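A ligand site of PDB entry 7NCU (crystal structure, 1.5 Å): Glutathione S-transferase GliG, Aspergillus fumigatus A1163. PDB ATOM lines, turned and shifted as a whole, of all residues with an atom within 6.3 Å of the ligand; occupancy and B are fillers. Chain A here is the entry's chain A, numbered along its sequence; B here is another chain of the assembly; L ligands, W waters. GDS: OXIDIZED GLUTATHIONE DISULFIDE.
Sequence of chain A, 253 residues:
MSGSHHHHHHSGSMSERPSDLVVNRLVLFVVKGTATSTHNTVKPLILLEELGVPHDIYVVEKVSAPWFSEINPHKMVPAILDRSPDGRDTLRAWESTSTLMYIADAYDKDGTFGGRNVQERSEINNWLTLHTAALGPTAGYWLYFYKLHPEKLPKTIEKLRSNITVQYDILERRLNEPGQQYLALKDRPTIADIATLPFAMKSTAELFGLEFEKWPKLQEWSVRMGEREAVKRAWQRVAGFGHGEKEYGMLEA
N of Ser 96 sits at hydrogen-bond distance from OE8 of the ligand. An oxygen (OE7) of the ligand is in hydrogen-bond range of the side-chain hydroxyl (OG) of Ser 96, 2.6 Å away. N6 of the ligand is in salt-bridge range of OE1 of Glu 95, 2.7 Å away. The backbone NH of Val 77 lies within hydrogen-bond range of an oxygen (O5) of the ligand (3.0 Å). The backbone carbonyl oxygen of Val 77 is in hydrogen-bond range of a nitrogen (N5) of the ligand. An oxygen (OE7) of the ligand sits close to the side-chain amide oxygen (OD1) of Asn 40.
OD1 of Asn 40 is in hydrogen-bond range of OG of Ser 96 (3.4 Å). ND1 of His 74 is in hydrogen-bond range of OE2 of Glu 95. The side-chain amide oxygen of Asn 40 lies within hydrogen-bond range of the side-chain amino group of Lys 43 (3.0 Å). The backbone NH (N) of Ser 37 sits at hydrogen-bond distance from the side-chain hydroxyl (OG1) of Thr 34, at 2.9 Å. O of Lys 32 is in hydrogen-bond range of OG of Ser 37 (2.8 Å). The backbone NH (N) of Thr 36 lies close to the side-chain hydroxyl (OG1) of Thr 34 (3.1 Å).
The side-chain sulfur (SD) of Met 76 sits close to an oxygen (O6) of the ligand (3.7 Å). Merely in contact with the ligand: Ser 37, Pro 78, Val 31, Thr 36 and Lys 75. Hydrophobic or aromatic side chains within 4 Å of the ligand: Val 31, Met 76, Val 77 and Pro 78. The nearest printed residue that does not touch the ligand is Val 63 (4.05 Å).
Water W3 lies within hydrogen-bond range of an oxygen (O1) of the ligand (2.4 Å) and the backbone carbonyl oxygen (O) of Lys 32 (2.8 Å). Water W2 lies within hydrogen-bond range of the side-chain hydroxyl of Thr 34 (2.9 Å) and an oxygen (O1) of the ligand (3.0 Å). Water W6 lies within hydrogen-bond range of the backbone carbonyl oxygen of Pro 78 (2.7 Å), an oxygen (OE8) of the ligand (2.8 Å) and the backbone NH of Glu 95 (3.2 Å). Water W9 bridges ND2 of Asn 40 and N5 of the ligand. Water W10 bridges the backbone carbonyl oxygen (O) of Ala 133 of chain B (2.8 Å) and a nitrogen (N6) of the ligand (3.5 Å). Water W8 lies within hydrogen-bond range of the side-chain carboxylate (OE1) of Glu 95 (2.8 Å), the backbone NH (N) of Thr 97 (3.0 Å), the backbone NH (N) of Ser 96 (3.5 Å) and an oxygen (OE7) of the ligand (3.5 Å).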
ATOM      1  N   VAL A  31     -31.690  -0.492  19.953  1.00  0.00           N
ATOM      2  CA  VAL A  31     -32.816  -1.459  20.066  1.00  0.00           C
ATOM      3  C   VAL A  31     -32.353  -2.568  21.017  1.00  0.00           C
ATOM      4  O   VAL A  31     -31.198  -2.580  21.399  1.00  0.00           O
ATOM      5  CB  VAL A  31     -33.263  -2.013  18.694  1.00  0.00           C
ATOM      6  CG1 VAL A  31     -33.933  -0.946  17.853  1.00  0.00           C
ATOM      7  CG2 VAL A  31     -32.120  -2.692  17.943  1.00  0.00           C
ATOM      8  N   LYS A  32     -33.255  -3.475  21.372  1.00  0.00           N
ATOM      9  CA  LYS A  32     -32.907  -4.589  22.283  1.00  0.00           C
ATOM     10  C   LYS A  32     -31.696  -5.326  21.708  1.00  0.00           C
ATOM     11  O   LYS A  32     -31.670  -5.583  20.504  1.00  0.00           O
ATOM     12  CB  LYS A  32     -34.105  -5.504  22.455  1.00  0.00           C
ATOM     13  CG  LYS A  32     -33.909  -6.637  23.454  1.00  0.00           C
ATOM     14  CD  LYS A  32     -35.187  -7.402  23.740  1.00  0.00           C
ATOM     15  CE  LYS A  32     -34.997  -8.489  24.767  1.00  0.00           C
ATOM     16  NZ  LYS A  32     -36.267  -9.231  24.999  1.00  0.00           N
ATOM     17  N   GLY A  33     -30.721  -5.633  22.554  1.00  0.00           N
ATOM     18  CA  GLY A  33     -29.492  -6.311  22.103  1.00  0.00           C
ATOM     19  C   GLY A  33     -29.784  -7.717  21.581  1.00  0.00           C
ATOM     20  O   GLY A  33     -30.491  -8.461  22.265  1.00  0.00           O
ATOM     21  N   THR A  34     -29.273  -8.041  20.389  1.00  0.00           N
ATOM     22  CA  THR A  34     -29.166  -9.415  19.836  1.00  0.00           C
ATOM     23  C   THR A  34     -27.761  -9.623  19.254  1.00  0.00           C
ATOM     24  O   THR A  34     -26.991  -8.652  19.202  1.00  0.00           O
ATOM     25  CB  THR A  34     -30.227  -9.701  18.760  1.00  0.00           C
ATOM     26  OG1 THR A  34     -29.828  -9.083  17.539  1.00  0.00           O
ATOM     27  CG2 THR A  34     -31.605  -9.232  19.183  1.00  0.00           C
ATOM     28  N   THR A  36     -27.039  -9.805  16.293  1.00  0.00           N
ATOM     29  CA  THR A  36     -26.981  -9.017  15.025  1.00  0.00           C
ATOM     30  C   THR A  36     -27.535  -7.595  15.163  1.00  0.00           C
ATOM     31  O   THR A  36     -27.570  -6.892  14.142  1.00  0.00           O
ATOM     32  CB  THR A  36     -27.808  -9.654  13.908  1.00  0.00           C
ATOM     33  OG1 THR A  36     -27.769 -11.080  14.043  1.00  0.00           O
ATOM     34  CG2 THR A  36     -27.307  -9.256  12.525  1.00  0.00           C
ATOM     35  N   SER A  37     -27.976  -7.154  16.342  1.00  0.00           N
ATOM     36  CA  SER A  37     -28.658  -5.828  16.440  1.00  0.00           C
ATOM     37  C   SER A  37     -27.656  -4.736  16.825  1.00  0.00           C
ATOM     38  O   SER A  37     -28.082  -3.576  16.974  1.00  0.00           O
ATOM     39  CB  SER A  37     -29.832  -5.882  17.390  1.00  0.00           C
ATOM     40  OG  SER A  37     -29.454  -5.613  18.728  1.00  0.00           O
ATOM     41  N   THR A  38     -26.377  -5.055  17.039  1.00  0.00           N
ATOM     42  CA  THR A  38     -25.467  -4.132  17.761  1.00  0.00           C
ATOM     43  C   THR A  38     -24.242  -3.684  16.951  1.00  0.00           C
ATOM     44  O   THR A  38     -23.504  -2.875  17.508  1.00  0.00           O
ATOM     45  CB  THR A  38     -25.018  -4.734  19.109  1.00  0.00           C
ATOM     46  OG1 THR A  38     -24.118  -5.820  18.882  1.00  0.00           O
ATOM     47  CG2 THR A  38     -26.194  -5.168  19.950  1.00  0.00           C
ATOM     48  N   ASN A  40     -23.849  -1.621  14.529  1.00  0.00           N
ATOM     49  CA  ASN A  40     -23.841  -0.156  14.230  1.00  0.00           C
ATOM     50  C   ASN A  40     -24.014   0.658  15.525  1.00  0.00           C
ATOM     51  O   ASN A  40     -23.325   1.678  15.655  1.00  0.00           O
ATOM     52  CB  ASN A  40     -24.792   0.192  13.081  1.00  0.00           C
ATOM     53  CG  ASN A  40     -24.188  -0.229  11.750  1.00  0.00           C
ATOM     54  OD1 ASN A  40     -23.063   0.155  11.401  1.00  0.00           O
ATOM     55  ND2 ASN A  40     -24.906  -1.076  11.029  1.00  0.00           N
ATOM     56  N   THR A  41     -24.881   0.250  16.442  1.00  0.00           N
ATOM     57  CA  THR A  41     -25.136   1.007  17.695  1.00  0.00           C
ATOM     58  C   THR A  41     -23.882   1.009  18.578  1.00  0.00           C
ATOM     59  O   THR A  41     -23.671   1.970  19.316  1.00  0.00           O
ATOM     60  CB  THR A  41     -26.379   0.509  18.421  1.00  0.00           C
ATOM     61  OG1 THR A  41     -26.265  -0.905  18.572  1.00  0.00           O
ATOM     62  CG2 THR A  41     -27.650   0.842  17.685  1.00  0.00           C
ATOM     63  N   LYS A  43     -20.926   1.522  17.779  1.00  0.00           N
ATOM     64  CA  LYS A  43     -19.894   2.462  17.246  1.00  0.00           C
ATOM     65  C   LYS A  43     -19.932   3.758  18.070  1.00  0.00           C
ATOM     66  O   LYS A  43     -18.932   4.099  18.713  1.00  0.00           O
ATOM     67  CB  LYS A  43     -20.066   2.678  15.740  1.00  0.00           C
ATOM     68  CG  LYS A  43     -19.814   1.438  14.875  1.00  0.00           C
ATOM     69  CD  LYS A  43     -20.200   1.636  13.428  1.00  0.00           C
ATOM     70  CE  LYS A  43     -19.921   0.463  12.532  1.00  0.00           C
ATOM     71  NZ  LYS A  43     -20.136   0.795  11.106  1.00  0.00           N
ATOM     72  N   VAL A  63     -39.037   1.135  15.596  1.00  0.00           N
ATOM     73  CA  VAL A  63     -38.325   2.183  14.823  1.00  0.00           C
ATOM     74  C   VAL A  63     -39.282   2.784  13.787  1.00  0.00           C
ATOM     75  O   VAL A  63     -38.931   3.822  13.221  1.00  0.00           O
ATOM     76  CB  VAL A  63     -37.046   1.645  14.139  1.00  0.00           C
ATOM     77  CG1 VAL A  63     -36.002   1.267  15.172  1.00  0.00           C
ATOM     78  CG2 VAL A  63     -37.337   0.496  13.177  1.00  0.00           C
ATOM     79  N   HIS A  74     -34.602   7.721   8.221  1.00  0.00           N
ATOM     80  CA  HIS A  74     -34.242   6.367   7.714  1.00  0.00           C
ATOM     81  C   HIS A  74     -34.728   5.290   8.694  1.00  0.00           C
ATOM     82  O   HIS A  74     -34.611   4.112   8.336  1.00  0.00           O
ATOM     83  CB  HIS A  74     -32.730   6.325   7.446  1.00  0.00           C
ATOM     84  CG  HIS A  74     -32.317   5.331   6.420  1.00  0.00           C
ATOM     85  ND1 HIS A  74     -30.998   5.123   6.098  1.00  0.00           N
ATOM     86  CD2 HIS A  74     -33.027   4.452   5.670  1.00  0.00           C
ATOM     87  CE1 HIS A  74     -30.907   4.172   5.185  1.00  0.00           C
ATOM     88  NE2 HIS A  74     -32.134   3.742   4.904  1.00  0.00           N
ATOM     89  N   LYS A  75     -35.239   5.656   9.871  1.00  0.00           N
ATOM     90  CA  LYS A  75     -35.940   4.728  10.794  1.00  0.00           C
ATOM     91  C   LYS A  75     -34.986   3.616  11.243  1.00  0.00           C
ATOM     92  O   LYS A  75     -35.381   2.444  11.258  1.00  0.00           O
ATOM     93  CB  LYS A  75     -37.191   4.183  10.109  1.00  0.00           C
ATOM     94  CG  LYS A  75     -38.194   5.260   9.723  1.00  0.00           C
ATOM     95  CD  LYS A  75     -39.506   4.718   9.191  1.00  0.00           C
ATOM     96  CE  LYS A  75     -39.375   4.153   7.801  1.00  0.00           C
ATOM     97  NZ  LYS A  75     -40.603   3.439   7.371  1.00  0.00           N
ATOM     98  N   MET A  76     -33.754   3.967  11.591  1.00  0.00           N
ATOM     99  CA  MET A  76     -32.778   2.966  12.088  1.00  0.00           C
ATOM    100  C   MET A  76     -32.068   3.520  13.313  1.00  0.00           C
ATOM    101  O   MET A  76     -32.021   4.759  13.505  1.00  0.00           O
ATOM    102  CB  MET A  76     -31.755   2.561  11.019  1.00  0.00           C
ATOM    103  CG  MET A  76     -32.384   1.864   9.822  1.00  0.00           C
ATOM    104  SD  MET A  76     -31.173   1.165   8.674  1.00  0.00           S
ATOM    105  CE  MET A  76     -30.664   2.627   7.800  1.00  0.00           C
ATOM    106  N   VAL A  77     -31.482   2.623  14.092  1.00  0.00           N
ATOM    107  CA  VAL A  77     -30.529   2.973  15.181  1.00  0.00           C
ATOM    108  C   VAL A  77     -29.120   2.657  14.669  1.00  0.00           C
ATOM    109  O   VAL A  77     -28.914   1.763  13.823  1.00  0.00           O
ATOM    110  CB  VAL A  77     -30.889   2.263  16.505  1.00  0.00           C
ATOM    111  CG1 VAL A  77     -32.235   2.781  17.010  1.00  0.00           C
ATOM    112  CG2 VAL A  77     -30.891   0.738  16.391  1.00  0.00           C
ATOM    113  N   PRO A  78     -28.088   3.371  15.133  1.00  0.00           N
ATOM    114  CA  PRO A  78     -28.219   4.399  16.158  1.00  0.00           C
ATOM    115  C   PRO A  78     -28.713   5.768  15.689  1.00  0.00           C
ATOM    116  O   PRO A  78     -28.621   6.114  14.504  1.00  0.00           O
ATOM    117  CB  PRO A  78     -26.772   4.582  16.656  1.00  0.00           C
ATOM    118  CG  PRO A  78     -25.934   4.266  15.438  1.00  0.00           C
ATOM    119  CD  PRO A  78     -26.680   3.152  14.745  1.00  0.00           C
ATOM    120  N   TRP A  94     -27.743  10.954  13.147  1.00  0.00           N
ATOM    121  CA  TRP A  94     -28.212   9.614  12.700  1.00  0.00           C
ATOM    122  C   TRP A  94     -27.396   9.186  11.485  1.00  0.00           C
ATOM    123  O   TRP A  94     -26.836  10.067  10.815  1.00  0.00           O
ATOM    124  CB  TRP A  94     -29.729   9.593  12.445  1.00  0.00           C
ATOM    125  CG  TRP A  94     -30.249  10.821  11.748  1.00  0.00           C
ATOM    126  CD1 TRP A  94     -30.790  11.918  12.359  1.00  0.00           C
ATOM    127  CD2 TRP A  94     -30.369  11.050  10.334  1.00  0.00           C
ATOM    128  NE1 TRP A  94     -31.156  12.844  11.417  1.00  0.00           N
ATOM    129  CE2 TRP A  94     -30.925  12.344  10.167  1.00  0.00           C
ATOM    130  CE3 TRP A  94     -30.050  10.314   9.190  1.00  0.00           C
ATOM    131  CZ2 TRP A  94     -31.169  12.894   8.910  1.00  0.00           C
ATOM    132  CZ3 TRP A  94     -30.278  10.863   7.941  1.00  0.00           C
ATOM    133  CH2 TRP A  94     -30.837  12.139   7.807  1.00  0.00           C
ATOM    134  N   GLU A  95     -27.384   7.867  11.239  1.00  0.00           N
ATOM    135  CA  GLU A  95     -26.303   7.104  10.546  1.00  0.00           C
ATOM    136  C   GLU A  95     -25.128   6.963  11.527  1.00  0.00           C
ATOM    137  O   GLU A  95     -24.666   7.998  12.061  1.00  0.00           O
ATOM    138  CB  GLU A  95     -25.893   7.777   9.237  1.00  0.00           C
ATOM    139  CG  GLU A  95     -26.815   7.432   8.071  1.00  0.00           C
ATOM    140  CD  GLU A  95     -26.842   5.939   7.755  1.00  0.00           C
ATOM    141  OE1 GLU A  95     -25.759   5.274   7.807  1.00  0.00           O
ATOM    142  OE2 GLU A  95     -27.942   5.421   7.449  1.00  0.00           O
ATOM    143  N   SER A  96     -24.616   5.747  11.745  1.00  0.00           N
ATOM    144  CA  SER A  96     -23.564   5.509  12.764  1.00  0.00           C
ATOM    145  C   SER A  96     -22.346   6.407  12.498  1.00  0.00           C
ATOM    146  O   SER A  96     -21.766   6.930  13.474  1.00  0.00           O
ATOM    147  CB  SER A  96     -23.157   4.050  12.838  1.00  0.00           C
ATOM    148  OG  SER A  96     -22.742   3.567  11.565  1.00  0.00           O
ATOM    149  N   THR A  97     -21.924   6.580  11.250  1.00  0.00           N
ATOM    150  CA  THR A  97     -20.740   7.440  10.931  1.00  0.00           C
ATOM    151  C   THR A  97     -21.034   8.884  11.369  1.00  0.00           C
ATOM    152  O   THR A  97     -20.154   9.506  11.989  1.00  0.00           O
ATOM    153  CB  THR A  97     -20.323   7.343   9.462  1.00  0.00           C
ATOM    154  OG1 THR A  97     -19.632   6.093   9.347  1.00  0.00           O
ATOM    155  CG2 THR A  97     -19.411   8.477   9.035  1.00  0.00           C
ATOM    156  N   LEU A 148     -32.830 -10.911   6.685  1.00  0.00           N
ATOM    157  CA  LEU A 148     -34.089 -10.114   6.733  1.00  0.00           C
ATOM    158  C   LEU A 148     -34.918 -10.289   5.455  1.00  0.00           C
ATOM    159  O   LEU A 148     -36.166 -10.232   5.575  1.00  0.00           O
ATOM    160  CB  LEU A 148     -33.757  -8.642   6.989  1.00  0.00           C
ATOM    161  CG  LEU A 148     -32.906  -8.351   8.222  1.00  0.00           C
ATOM    162  CD1 LEU A 148     -32.674  -6.854   8.391  1.00  0.00           C
ATOM    163  CD2 LEU A 148     -33.535  -8.946   9.481  1.00  0.00           C
ATOM    164  N   ALA B 133     -23.704   6.477   2.788  1.00  0.00           N
ATOM    165  CA  ALA B 133     -24.013   5.119   3.303  1.00  0.00           C
ATOM    166  C   ALA B 133     -25.205   4.510   2.572  1.00  0.00           C
ATOM    167  O   ALA B 133     -25.277   3.265   2.528  1.00  0.00           O
ATOM    168  CB  ALA B 133     -24.234   5.173   4.803  1.00  0.00           C
HETATM  169  CD1 GDS L   1     -33.700  -6.826  15.664  1.00  0.00           C
HETATM  170  O1  GDS L   1     -32.958  -6.312  16.490  1.00  0.00           O
HETATM  171  N2  GDS L   1     -33.559  -6.629  14.360  1.00  0.00           N
HETATM  172  CA2 GDS L   1     -33.405  -5.298  13.783  1.00  0.00           C
HETATM  173  C2  GDS L   1     -34.737  -4.605  13.435  1.00  0.00           C
HETATM  174  O2  GDS L   1     -35.059  -4.435  12.254  1.00  0.00           O
HETATM  175  CB2 GDS L   1     -32.445  -5.324  12.611  1.00  0.00           C
HETATM  176  SG2 GDS L   1     -30.761  -5.008  13.230  1.00  0.00           S
HETATM  177  N3  GDS L   1     -35.518  -4.239  14.456  1.00  0.00           N
HETATM  178  N4  GDS L   1     -32.647  -1.637  11.549  1.00  0.00           N
HETATM  179  CA4 GDS L   1     -34.042  -1.294  11.445  1.00  0.00           C
HETATM  180  C4  GDS L   1     -34.724  -1.973  10.267  1.00  0.00           C
HETATM  181  OE5 GDS L   1     -34.022  -2.734   9.538  1.00  0.00           O
HETATM  182  OE6 GDS L   1     -35.935  -1.745  10.110  1.00  0.00           O
HETATM  183  C5  GDS L   1     -31.841  -1.042  12.429  1.00  0.00           C
HETATM  184  O5  GDS L   1     -32.206  -0.120  13.177  1.00  0.00           O
HETATM  185  CA5 GDS L   1     -30.384  -1.510  12.441  1.00  0.00           C
HETATM  186  N5  GDS L   1     -29.460  -0.439  12.109  1.00  0.00           N
HETATM  187  CB5 GDS L   1     -30.015  -2.063  13.809  1.00  0.00           C
HETATM  188  SG5 GDS L   1     -31.097  -3.385  14.413  1.00  0.00           S
HETATM  189  CA6 GDS L   1     -26.808   2.507   9.170  1.00  0.00           C
HETATM  190  C6  GDS L   1     -25.758   2.918  10.207  1.00  0.00           C
HETATM  191  OE7 GDS L   1     -24.576   2.626   9.966  1.00  0.00           O
HETATM  192  OE8 GDS L   1     -26.148   3.478  11.255  1.00  0.00           O
HETATM  193  N6  GDS L   1     -26.233   2.596   7.800  1.00  0.00           N
HETATM  194  CB6 GDS L   1     -27.342   1.089   9.444  1.00  0.00           C
HETATM  195  CG6 GDS L   1     -27.964   0.931  10.817  1.00  0.00           C
HETATM  196  CD6 GDS L   1     -28.768  -0.342  10.962  1.00  0.00           C
HETATM  197  O6  GDS L   1     -28.772  -1.220  10.101  1.00  0.00           O
HETATM  198  O   HOH W   1     -31.151  -3.202   9.366  1.00  0.00           O
HETATM  199  O   HOH W   2     -31.878  -8.919  15.476  1.00  0.00           O
HETATM  200  O   HOH W   3     -33.808  -5.996  18.759  1.00  0.00           O
HETATM  201  O   HOH W   4     -27.732   3.228   5.572  1.00  0.00           O
HETATM  202  O   HOH W   5     -27.555  -2.126   7.737  1.00  0.00           O
HETATM  203  O   HOH W   6     -28.414   4.955  12.051  1.00  0.00           O
HETATM  204  O   HOH W   7     -24.011   1.092   6.841  1.00  0.00           O
HETATM  205  O   HOH W   8     -23.051   5.486   8.655  1.00  0.00           O
HETATM  206  O   HOH W   9     -26.801  -2.644  12.641  1.00  0.00           O
HETATM  207  O   HOH W  10     -25.331   1.453   4.636  1.00  0.00           O
HETATM  208  O   HOH W  11     -36.690   0.685   9.658  1.00  0.00           O
